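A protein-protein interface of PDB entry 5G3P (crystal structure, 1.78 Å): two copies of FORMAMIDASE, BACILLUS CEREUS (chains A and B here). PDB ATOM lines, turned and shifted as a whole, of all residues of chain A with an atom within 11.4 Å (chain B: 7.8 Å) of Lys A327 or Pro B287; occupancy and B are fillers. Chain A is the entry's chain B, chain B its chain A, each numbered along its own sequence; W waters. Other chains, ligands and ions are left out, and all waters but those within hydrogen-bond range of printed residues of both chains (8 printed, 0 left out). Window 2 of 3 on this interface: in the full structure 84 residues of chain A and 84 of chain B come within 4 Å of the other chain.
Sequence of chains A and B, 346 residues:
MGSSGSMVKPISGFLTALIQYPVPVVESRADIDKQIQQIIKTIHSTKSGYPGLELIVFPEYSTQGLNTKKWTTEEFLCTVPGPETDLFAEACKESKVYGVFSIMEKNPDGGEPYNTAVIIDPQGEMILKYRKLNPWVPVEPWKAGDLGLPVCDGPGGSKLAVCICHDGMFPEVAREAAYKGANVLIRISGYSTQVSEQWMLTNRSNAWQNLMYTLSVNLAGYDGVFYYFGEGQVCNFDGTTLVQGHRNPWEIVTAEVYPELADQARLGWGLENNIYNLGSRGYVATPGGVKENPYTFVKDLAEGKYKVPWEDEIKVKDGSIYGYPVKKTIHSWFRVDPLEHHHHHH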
ATOM      1  N   GLY A 111     -11.640  -6.989  17.221  1.00  0.00           N
ATOM      2  CA  GLY A 111     -12.272  -5.801  16.675  1.00  0.00           C
ATOM      3  C   GLY A 111     -12.087  -4.588  17.532  1.00  0.00           C
ATOM      4  O   GLY A 111     -11.193  -4.536  18.389  1.00  0.00           O
ATOM      5  N   GLU A 112     -12.980  -3.626  17.380  1.00  0.00           N
ATOM      6  CA  GLU A 112     -12.819  -2.381  18.092  1.00  0.00           C
ATOM      7  C   GLU A 112     -13.082  -2.574  19.590  1.00  0.00           C
ATOM      8  O   GLU A 112     -13.959  -3.352  19.986  1.00  0.00           O
ATOM      9  CB  GLU A 112     -13.737  -1.304  17.499  1.00  0.00           C
ATOM     10  CG  GLU A 112     -13.430  -1.005  16.006  1.00  0.00           C
ATOM     11  CD  GLU A 112     -12.015  -0.499  15.790  1.00  0.00           C
ATOM     12  OE1 GLU A 112     -11.505   0.269  16.616  1.00  0.00           O
ATOM     13  OE2 GLU A 112     -11.379  -0.909  14.814  1.00  0.00           O
ATOM     14  N   PRO A 135     -21.314   5.274  22.917  1.00  0.00           N
ATOM     15  CA  PRO A 135     -20.059   6.035  22.848  1.00  0.00           C
ATOM     16  C   PRO A 135     -20.292   7.508  22.440  1.00  0.00           C
ATOM     17  O   PRO A 135     -21.277   7.838  21.737  1.00  0.00           O
ATOM     18  CB  PRO A 135     -19.277   5.295  21.774  1.00  0.00           C
ATOM     19  CG  PRO A 135     -19.750   3.886  21.912  1.00  0.00           C
ATOM     20  CD  PRO A 135     -21.217   3.995  22.217  1.00  0.00           C
ATOM     21  N   VAL A 137     -19.716   9.917  20.363  1.00  0.00           N
ATOM     22  CA  VAL A 137     -19.325  10.122  18.987  1.00  0.00           C
ATOM     23  C   VAL A 137     -19.484  11.606  18.605  1.00  0.00           C
ATOM     24  O   VAL A 137     -20.457  12.247  19.017  1.00  0.00           O
ATOM     25  CB  VAL A 137     -20.114   9.214  18.031  1.00  0.00           C
ATOM     26  CG1 VAL A 137     -19.721   7.753  18.263  1.00  0.00           C
ATOM     27  CG2 VAL A 137     -21.640   9.391  18.145  1.00  0.00           C
ATOM     28  N   GLU A 140     -15.175   9.580  20.362  1.00  0.00           N
ATOM     29  CA  GLU A 140     -14.854   8.265  20.931  1.00  0.00           C
ATOM     30  C   GLU A 140     -14.883   7.137  19.896  1.00  0.00           C
ATOM     31  O   GLU A 140     -15.798   7.044  19.090  1.00  0.00           O
ATOM     32  CB  GLU A 140     -15.792   7.960  22.072  1.00  0.00           C
ATOM     33  CG  GLU A 140     -15.496   8.783  23.315  1.00  0.00           C
ATOM     34  CD  GLU A 140     -16.311   8.370  24.509  1.00  0.00           C
ATOM     35  OE1 GLU A 140     -17.217   7.495  24.400  1.00  0.00           O
ATOM     36  OE2 GLU A 140     -16.066   8.967  25.585  1.00  0.00           O
ATOM     37  N   PRO A 141     -13.873   6.241  19.942  1.00  0.00           N
ATOM     38  CA  PRO A 141     -13.745   5.167  18.973  1.00  0.00           C
ATOM     39  C   PRO A 141     -14.378   3.847  19.447  1.00  0.00           C
ATOM     40  O   PRO A 141     -14.310   2.878  18.732  1.00  0.00           O
ATOM     41  CB  PRO A 141     -12.215   5.008  18.870  1.00  0.00           C
ATOM     42  CG  PRO A 141     -11.758   5.246  20.280  1.00  0.00           C
ATOM     43  CD  PRO A 141     -12.654   6.369  20.775  1.00  0.00           C
ATOM     44  N   TRP A 142     -14.994   3.822  20.630  1.00  0.00           N
ATOM     45  CA  TRP A 142     -15.406   2.590  21.278  1.00  0.00           C
ATOM     46  C   TRP A 142     -16.561   1.921  20.522  1.00  0.00           C
ATOM     47  O   TRP A 142     -17.453   2.600  19.958  1.00  0.00           O
ATOM     48  CB  TRP A 142     -15.817   2.817  22.725  1.00  0.00           C
ATOM     49  CG  TRP A 142     -14.848   3.676  23.444  1.00  0.00           C
ATOM     50  CD1 TRP A 142     -15.073   4.924  23.938  1.00  0.00           C
ATOM     51  CD2 TRP A 142     -13.470   3.390  23.674  1.00  0.00           C
ATOM     52  NE1 TRP A 142     -13.921   5.429  24.479  1.00  0.00           N
ATOM     53  CE2 TRP A 142     -12.918   4.510  24.331  1.00  0.00           C
ATOM     54  CE3 TRP A 142     -12.649   2.291  23.405  1.00  0.00           C
ATOM     55  CZ2 TRP A 142     -11.569   4.571  24.709  1.00  0.00           C
ATOM     56  CZ3 TRP A 142     -11.307   2.338  23.792  1.00  0.00           C
ATOM     57  CH2 TRP A 142     -10.782   3.467  24.457  1.00  0.00           C
ATOM     58  N   LYS A 143     -16.533   0.597  20.522  1.00  0.00           N
ATOM     59  CA  LYS A 143     -17.601  -0.198  19.962  1.00  0.00           C
ATOM     60  C   LYS A 143     -18.844  -0.066  20.826  1.00  0.00           C
ATOM     61  O   LYS A 143     -18.758  -0.077  22.039  1.00  0.00           O
ATOM     62  CB  LYS A 143     -17.183  -1.663  19.867  1.00  0.00           C
ATOM     63  CG  LYS A 143     -18.218  -2.545  19.196  1.00  0.00           C
ATOM     64  CD  LYS A 143     -17.721  -3.956  18.998  1.00  0.00           C
ATOM     65  CE  LYS A 143     -18.834  -4.839  18.397  1.00  0.00           C
ATOM     66  NZ  LYS A 143     -19.136  -4.496  16.987  1.00  0.00           N
ATOM     67  N   ALA A 144     -20.004   0.052  20.188  1.00  0.00           N
ATOM     68  CA  ALA A 144     -21.260   0.142  20.917  1.00  0.00           C
ATOM     69  C   ALA A 144     -21.436  -1.117  21.754  1.00  0.00           C
ATOM     70  O   ALA A 144     -21.226  -2.251  21.283  1.00  0.00           O
ATOM     71  CB  ALA A 144     -22.418   0.280  19.935  1.00  0.00           C
ATOM     72  N   GLU A 311     -32.464  12.438   8.715  1.00  0.00           N
ATOM     73  CA  GLU A 311     -31.186  11.730   8.809  1.00  0.00           C
ATOM     74  C   GLU A 311     -30.248  11.953   7.617  1.00  0.00           C
ATOM     75  O   GLU A 311     -29.044  12.087   7.816  1.00  0.00           O
ATOM     76  CB  GLU A 311     -31.369  10.224   8.986  1.00  0.00           C
ATOM     77  CG  GLU A 311     -30.104   9.528   9.485  1.00  0.00           C
ATOM     78  CD  GLU A 311     -30.192   8.027   9.364  1.00  0.00           C
ATOM     79  OE1 GLU A 311     -30.091   7.546   8.235  1.00  0.00           O
ATOM     80  OE2 GLU A 311     -30.404   7.352  10.386  1.00  0.00           O
ATOM     81  N   VAL A 316     -22.583  15.225  10.567  1.00  0.00           N
ATOM     82  CA  VAL A 316     -21.573  14.465  11.278  1.00  0.00           C
ATOM     83  C   VAL A 316     -22.075  13.032  11.476  1.00  0.00           C
ATOM     84  O   VAL A 316     -22.903  12.769  12.339  1.00  0.00           O
ATOM     85  CB  VAL A 316     -21.178  15.129  12.609  1.00  0.00           C
ATOM     86  CG1 VAL A 316     -20.064  14.353  13.306  1.00  0.00           C
ATOM     87  CG2 VAL A 316     -20.729  16.552  12.356  1.00  0.00           C
ATOM     88  N   LYS A 317     -21.540  12.112  10.664  1.00  0.00           N
ATOM     89  CA  LYS A 317     -21.897  10.693  10.691  1.00  0.00           C
ATOM     90  C   LYS A 317     -20.705   9.747  10.773  1.00  0.00           C
ATOM     91  O   LYS A 317     -20.877   8.534  10.668  1.00  0.00           O
ATOM     92  CB  LYS A 317     -22.668  10.364   9.413  1.00  0.00           C
ATOM     93  CG  LYS A 317     -24.067  10.946   9.387  1.00  0.00           C
ATOM     94  CD  LYS A 317     -24.716  10.594   8.056  1.00  0.00           C
ATOM     95  CE  LYS A 317     -26.198  10.767   8.158  1.00  0.00           C
ATOM     96  NZ  LYS A 317     -26.844  10.449   6.879  1.00  0.00           N
ATOM     97  N   ASP A 318     -19.504  10.280  10.955  1.00  0.00           N
ATOM     98  CA  ASP A 318     -18.301   9.437  11.089  1.00  0.00           C
ATOM     99  C   ASP A 318     -17.331  10.240  11.939  1.00  0.00           C
ATOM    100  O   ASP A 318     -17.670  11.355  12.365  1.00  0.00           O
ATOM    101  CB  ASP A 318     -17.733   9.059   9.715  1.00  0.00           C
ATOM    102  CG  ASP A 318     -17.387  10.288   8.855  1.00  0.00           C
ATOM    103  OD1 ASP A 318     -16.736  11.219   9.349  1.00  0.00           O
ATOM    104  OD2 ASP A 318     -17.758  10.299   7.672  1.00  0.00           O
ATOM    105  N   GLY A 319     -16.142   9.702  12.144  1.00  0.00           N
ATOM    106  CA  GLY A 319     -15.149  10.334  12.993  1.00  0.00           C
ATOM    107  C   GLY A 319     -14.163  11.228  12.274  1.00  0.00           C
ATOM    108  O   GLY A 319     -13.164  11.619  12.876  1.00  0.00           O
ATOM    109  N   SER A 320     -14.414  11.575  11.006  1.00  0.00           N
ATOM    110  CA  SER A 320     -13.425  12.329  10.203  1.00  0.00           C
ATOM    111  C   SER A 320     -13.108  13.724  10.767  1.00  0.00           C
ATOM    112  O   SER A 320     -11.958  14.186  10.679  1.00  0.00           O
ATOM    113  CB  SER A 320     -13.856  12.465   8.731  1.00  0.00           C
ATOM    114  OG  SER A 320     -15.103  13.148   8.629  1.00  0.00           O
ATOM    115  N   ILE A 321     -14.081  14.367  11.399  1.00  0.00           N
ATOM    116  CA  ILE A 321     -13.846  15.702  11.981  1.00  0.00           C
ATOM    117  C   ILE A 321     -12.777  15.670  13.081  1.00  0.00           C
ATOM    118  O   ILE A 321     -12.118  16.684  13.339  1.00  0.00           O
ATOM    119  CB  ILE A 321     -15.169  16.344  12.492  1.00  0.00           C
ATOM    120  CG1 ILE A 321     -15.012  17.845  12.721  1.00  0.00           C
ATOM    121  CG2 ILE A 321     -15.674  15.680  13.781  1.00  0.00           C
ATOM    122  CD1 ILE A 321     -16.352  18.553  12.873  1.00  0.00           C
ATOM    123  N   GLY A 323     -10.263  13.351  12.862  1.00  0.00           N
ATOM    124  CA  GLY A 323      -9.158  12.639  12.215  1.00  0.00           C
ATOM    125  C   GLY A 323      -9.228  11.114  12.190  1.00  0.00           C
ATOM    126  O   GLY A 323      -8.233  10.475  11.835  1.00  0.00           O
ATOM    127  N   TYR A 324     -10.365  10.509  12.552  1.00  0.00           N
ATOM    128  CA  TYR A 324     -10.530   9.054  12.398  1.00  0.00           C
ATOM    129  C   TYR A 324     -10.747   8.743  10.906  1.00  0.00           C
ATOM    130  O   TYR A 324     -11.568   9.395  10.269  1.00  0.00           O
ATOM    131  CB  TYR A 324     -11.704   8.499  13.206  1.00  0.00           C
ATOM    132  CG  TYR A 324     -11.511   8.565  14.697  1.00  0.00           C
ATOM    133  CD1 TYR A 324     -10.646   7.671  15.349  1.00  0.00           C
ATOM    134  CD2 TYR A 324     -12.213   9.506  15.476  1.00  0.00           C
ATOM    135  CE1 TYR A 324     -10.476   7.724  16.722  1.00  0.00           C
ATOM    136  CE2 TYR A 324     -12.054   9.557  16.846  1.00  0.00           C
ATOM    137  CZ  TYR A 324     -11.175   8.673  17.476  1.00  0.00           C
ATOM    138  OH  TYR A 324     -10.996   8.749  18.854  1.00  0.00           O
ATOM    139  N   PRO A 325      -9.999   7.766  10.348  1.00  0.00           N
ATOM    140  CA  PRO A 325     -10.284   7.363   8.952  1.00  0.00           C
ATOM    141  C   PRO A 325     -11.711   6.838   8.783  1.00  0.00           C
ATOM    142  O   PRO A 325     -12.267   6.266   9.733  1.00  0.00           O
ATOM    143  CB  PRO A 325      -9.251   6.254   8.667  1.00  0.00           C
ATOM    144  CG  PRO A 325      -8.170   6.423   9.674  1.00  0.00           C
ATOM    145  CD  PRO A 325      -8.752   7.157  10.865  1.00  0.00           C
ATOM    146  N   VAL A 326     -12.312   7.119   7.631  1.00  0.00           N
ATOM    147  CA  VAL A 326     -13.676   6.684   7.315  1.00  0.00           C
ATOM    148  C   VAL A 326     -13.652   5.402   6.462  1.00  0.00           C
ATOM    149  O   VAL A 326     -12.908   5.338   5.503  1.00  0.00           O
ATOM    150  CB  VAL A 326     -14.436   7.746   6.484  1.00  0.00           C
ATOM    151  CG1 VAL A 326     -15.881   7.304   6.236  1.00  0.00           C
ATOM    152  CG2 VAL A 326     -14.407   9.097   7.178  1.00  0.00           C
ATOM    153  N   LYS A 327     -14.472   4.406   6.807  1.00  0.00           N
ATOM    154  CA  LYS A 327     -14.841   3.296   5.885  1.00  0.00           C
ATOM    155  C   LYS A 327     -15.921   2.413   6.523  1.00  0.00           C
ATOM    156  O   LYS A 327     -16.797   1.871   5.838  1.00  0.00           O
ATOM    157  CB  LYS A 327     -13.630   2.412   5.454  1.00  0.00           C
ATOM    158  CG  LYS A 327     -12.778   2.828   4.235  1.00  0.00           C
ATOM    159  CD  LYS A 327     -13.498   3.588   3.113  1.00  0.00           C
ATOM    160  CE  LYS A 327     -12.543   4.461   2.308  1.00  0.00           C
ATOM    161  NZ  LYS A 327     -13.282   5.508   1.550  1.00  0.00           N
ATOM    162  N   TYR B 276     -30.260  11.747  17.122  1.00  0.00           N
ATOM    163  CA  TYR B 276     -29.705  10.851  16.130  1.00  0.00           C
ATOM    164  C   TYR B 276     -28.995   9.640  16.755  1.00  0.00           C
ATOM    165  O   TYR B 276     -29.174   8.506  16.309  1.00  0.00           O
ATOM    166  CB  TYR B 276     -28.739  11.625  15.233  1.00  0.00           C
ATOM    167  CG  TYR B 276     -27.955  10.783  14.244  1.00  0.00           C
ATOM    168  CD1 TYR B 276     -28.594   9.832  13.435  1.00  0.00           C
ATOM    169  CD2 TYR B 276     -26.578  10.952  14.100  1.00  0.00           C
ATOM    170  CE1 TYR B 276     -27.878   9.050  12.530  1.00  0.00           C
ATOM    171  CE2 TYR B 276     -25.860  10.197  13.187  1.00  0.00           C
ATOM    172  CZ  TYR B 276     -26.505   9.237  12.423  1.00  0.00           C
ATOM    173  OH  TYR B 276     -25.779   8.506  11.508  1.00  0.00           O
ATOM    174  N   ARG B 281     -25.649   3.653  17.133  1.00  0.00           N
ATOM    175  CA  ARG B 281     -24.697   3.742  18.236  1.00  0.00           C
ATOM    176  C   ARG B 281     -23.278   3.416  17.778  1.00  0.00           C
ATOM    177  O   ARG B 281     -23.057   2.546  16.936  1.00  0.00           O
ATOM    178  CB  ARG B 281     -25.111   2.778  19.356  1.00  0.00           C
ATOM    179  CG  ARG B 281     -26.539   3.000  19.834  1.00  0.00           C
ATOM    180  CD  ARG B 281     -26.911   2.064  20.967  1.00  0.00           C
ATOM    181  NE  ARG B 281     -27.126   0.686  20.524  1.00  0.00           N
ATOM    182  CZ  ARG B 281     -26.502  -0.412  20.945  1.00  0.00           C
ATOM    183  NH1 ARG B 281     -25.500  -0.377  21.816  1.00  0.00           N
ATOM    184  NH2 ARG B 281     -26.888  -1.582  20.465  1.00  0.00           N
ATOM    185  N   GLY B 282     -22.315   4.124  18.340  1.00  0.00           N
ATOM    186  CA  GLY B 282     -20.909   3.828  18.121  1.00  0.00           C
ATOM    187  C   GLY B 282     -20.505   3.864  16.649  1.00  0.00           C
ATOM    188  O   GLY B 282     -19.828   2.952  16.189  1.00  0.00           O
ATOM    189  N   TYR B 283     -20.913   4.918  15.933  1.00  0.00           N
ATOM    190  CA  TYR B 283     -20.649   4.994  14.493  1.00  0.00           C
ATOM    191  C   TYR B 283     -19.187   5.137  14.106  1.00  0.00           C
ATOM    192  O   TYR B 283     -18.848   4.943  12.944  1.00  0.00           O
ATOM    193  CB  TYR B 283     -21.542   6.009  13.743  1.00  0.00           C
ATOM    194  CG  TYR B 283     -21.405   7.447  14.116  1.00  0.00           C
ATOM    195  CD1 TYR B 283     -20.173   8.111  14.056  1.00  0.00           C
ATOM    196  CD2 TYR B 283     -22.521   8.184  14.508  1.00  0.00           C
ATOM    197  CE1 TYR B 283     -20.054   9.452  14.396  1.00  0.00           C
ATOM    198  CE2 TYR B 283     -22.413   9.537  14.829  1.00  0.00           C
ATOM    199  CZ  TYR B 283     -21.165  10.159  14.752  1.00  0.00           C
ATOM    200  OH  TYR B 283     -21.026  11.480  15.134  1.00  0.00           O
ATOM    201  N   VAL B 284     -18.301   5.504  15.033  1.00  0.00           N
ATOM    202  CA  VAL B 284     -16.868   5.529  14.679  1.00  0.00           C
ATOM    203  C   VAL B 284     -16.344   4.096  14.538  1.00  0.00           C
ATOM    204  O   VAL B 284     -15.645   3.793  13.575  1.00  0.00           O
ATOM    205  CB  VAL B 284     -16.042   6.386  15.672  1.00  0.00           C
ATOM    206  CG1 VAL B 284     -14.545   6.348  15.355  1.00  0.00           C
ATOM    207  CG2 VAL B 284     -16.566   7.818  15.653  1.00  0.00           C
ATOM    208  N   ALA B 285     -16.680   3.220  15.490  1.00  0.00           N
ATOM    209  CA  ALA B 285     -16.263   1.818  15.454  1.00  0.00           C
ATOM    210  C   ALA B 285     -17.029   0.994  14.402  1.00  0.00           C
ATOM    211  O   ALA B 285     -16.461   0.061  13.848  1.00  0.00           O
ATOM    212  CB  ALA B 285     -16.478   1.168  16.809  1.00  0.00           C
ATOM    213  N   THR B 286     -18.302   1.329  14.181  1.00  0.00           N
ATOM    214  CA  THR B 286     -19.170   0.624  13.242  1.00  0.00           C
ATOM    215  C   THR B 286     -19.767   1.648  12.282  1.00  0.00           C
ATOM    216  O   THR B 286     -20.702   2.333  12.641  1.00  0.00           O
ATOM    217  CB  THR B 286     -20.298  -0.119  13.993  1.00  0.00           C
ATOM    218  OG1 THR B 286     -19.721  -1.026  14.938  1.00  0.00           O
ATOM    219  CG2 THR B 286     -21.198  -0.910  13.015  1.00  0.00           C
ATOM    220  N   PRO B 287     -19.227   1.755  11.071  1.00  0.00           N
ATOM    221  CA  PRO B 287     -19.788   2.673  10.067  1.00  0.00           C
ATOM    222  C   PRO B 287     -21.304   2.593   9.926  1.00  0.00           C
ATOM    223  O   PRO B 287     -21.842   1.510   9.815  1.00  0.00           O
ATOM    224  CB  PRO B 287     -19.101   2.240   8.771  1.00  0.00           C
ATOM    225  CG  PRO B 287     -17.752   1.740   9.236  1.00  0.00           C
ATOM    226  CD  PRO B 287     -18.020   1.072  10.569  1.00  0.00           C
ATOM    227  N   GLY B 288     -21.975   3.729   9.978  1.00  0.00           N
ATOM    228  CA  GLY B 288     -23.437   3.779   9.962  1.00  0.00           C
ATOM    229  C   GLY B 288     -24.070   3.614  11.336  1.00  0.00           C
ATOM    230  O   GLY B 288     -25.250   3.909  11.496  1.00  0.00           O
ATOM    231  N   GLY B 289     -23.309   3.113  12.318  1.00  0.00           N
ATOM    232  CA  GLY B 289     -23.819   2.882  13.646  1.00  0.00           C
ATOM    233  C   GLY B 289     -24.455   1.507  13.825  1.00  0.00           C
ATOM    234  O   GLY B 289     -24.972   0.906  12.872  1.00  0.00           O
ATOM    235  N   VAL B 290     -24.413   1.016  15.062  1.00  0.00           N
ATOM    236  CA  VAL B 290     -25.082  -0.207  15.441  1.00  0.00           C
ATOM    237  C   VAL B 290     -26.574   0.121  15.594  1.00  0.00           C
ATOM    238  O   VAL B 290     -26.953   1.031  16.352  1.00  0.00           O
ATOM    239  CB  VAL B 290     -24.469  -0.770  16.737  1.00  0.00           C
ATOM    240  CG1 VAL B 290     -25.281  -1.949  17.262  1.00  0.00           C
ATOM    241  CG2 VAL B 290     -23.037  -1.222  16.463  1.00  0.00           C
ATOM    242  N   LYS B 291     -27.415  -0.638  14.898  1.00  0.00           N
ATOM    243  CA  LYS B 291     -28.848  -0.369  14.863  1.00  0.00           C
ATOM    244  C   LYS B 291     -29.680  -1.207  15.804  1.00  0.00           C
ATOM    245  O   LYS B 291     -30.808  -0.820  16.106  1.00  0.00           O
ATOM    246  CB  LYS B 291     -29.391  -0.637  13.446  1.00  0.00           C
ATOM    247  CG  LYS B 291     -28.752   0.189  12.335  1.00  0.00           C
ATOM    248  CD  LYS B 291     -28.945   1.688  12.460  1.00  0.00           C
ATOM    249  CE  LYS B 291     -30.407   2.102  12.255  1.00  0.00           C
ATOM    250  NZ  LYS B 291     -30.616   3.535  12.633  1.00  0.00           N
HETATM  251  O   HOH W   1     -17.307  -2.438  15.727  1.00  0.00           O
HETATM  252  O   HOH W   2     -22.978   6.219  20.166  1.00  0.00           O
HETATM  253  O   HOH W   3     -20.094   6.072  10.147  1.00  0.00           O
HETATM  254  O   HOH W   4     -19.908   0.400  17.333  1.00  0.00           O
HETATM  255  O   HOH W   5     -30.103   4.698  10.218  1.00  0.00           O
HETATM  256  O   HOH W   6     -23.331   7.018  10.916  1.00  0.00           O
HETATM  257  O   HOH W   7     -17.590   4.739  18.320  1.00  0.00           O
HETATM  258  O   HOH W   8     -20.972  -3.409  15.041  1.00  0.00           O
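The side-chain hydroxyl (OG) of Ser A320 lies within hydrogen-bond range of the side-chain carboxylate (OD1) of Asp A318.
The backbone carbonyl oxygen (O) of Glu A311 is in hydrogen-bond range of the side-chain amino group (NZ) of Lys A317, 2.9 Å away.
The backbone NH of Tyr A324 is in hydrogen-bond range of the backbone carbonyl oxygen of Gly A319 (3.0 Å).
The backbone NH (N) of Val B290 sits at hydrogen-bond distance from the backbone carbonyl oxygen (O) of Arg B281 (2.8 Å).
Glu A112 touches Ala B285 (CB to CB, 3.8 Å).
Gly B282 touches Pro A135.
Val B284 touches Glu A140.
CB of Ala B285 touches O of Trp A142 (3.6 Å).
CB of Ala B285 touches CA of Lys A143 (3.6 Å).
Ala A144 touches Arg B281 (CB to NH1, 3.7 Å).
OH of Tyr B283 touches CG1 of Val A316, 3.5 Å away.
Lys A317 touches Tyr B283.
N of Asp A318 touches CE1 of Tyr B283, 3.6 Å away.
CG1 of Val B284 touches CG of Tyr A324, at 3.8 Å.
Of the printed residues of chain B, Lys A327 touches Pro B287.
Of the printed residues of chain A, Pro B287 touches Lys A327.
No residue of chain A comes within 4 Å of Thr B286.
No residue of chain A comes within 4 Å of Gly B288.
No residue of chain A comes within 4 Å of Gly B289.
Of the printed residues of chain B, Trp A142 touches Ala B285.
Printed residues of chain A within 4 Å of Arg B281: Ala A144 (3.7 Å).
Pro A325 touches none of the printed residues of chain B.
The nearest residue of chain A that does not touch Pro B287 is Lys A317 (6.0 Å).
The nearest printed residue of chain A that does not touch Tyr B276 is Val A316 (4.01 Å).
Printed residues of chain B that touch a printed residue of chain A: Tyr B276, Arg B281, Gly B282, Tyr B283, Val B284, Ala B285, Pro B287 and Val B290.
Along chain B the printed residues that touch a printed residue of chain A span positions 276 to 290.
Of the 21 printed residues of chain A, 15 touch a printed residue of chain B.
No position is printed for both chains.
Water W8 bridges OG1 of Thr B286 (2.7 Å) and NZ of Lys A143 (2.9 Å).
Water W7 lies within hydrogen-bond range of the backbone carbonyl oxygen (O) of Trp A142, the backbone carbonyl oxygen (O) of Glu A140, the backbone NH (N) of Ala B285 and the backbone NH (N) of Val B284.
Water W4 lies within hydrogen-bond range of the side-chain hydroxyl (OG1) of Thr B286, the backbone carbonyl oxygen (O) of Gly B282 and the backbone NH (N) of Ala A144.
Water W2 bridges O of Pro A135 (2.8 Å) and N of Gly B282 (2.9 Å).
Water W6 bridges the backbone carbonyl oxygen (O) of Lys A317 (2.9 Å) and the side-chain hydroxyl (OH) of Tyr B276 (2.9 Å).
Water W1 lies within hydrogen-bond range of OG1 of Thr B286 (2.9 Å), NZ of Lys A143 (3.0 Å) and O of Ala B285 (3.2 Å).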
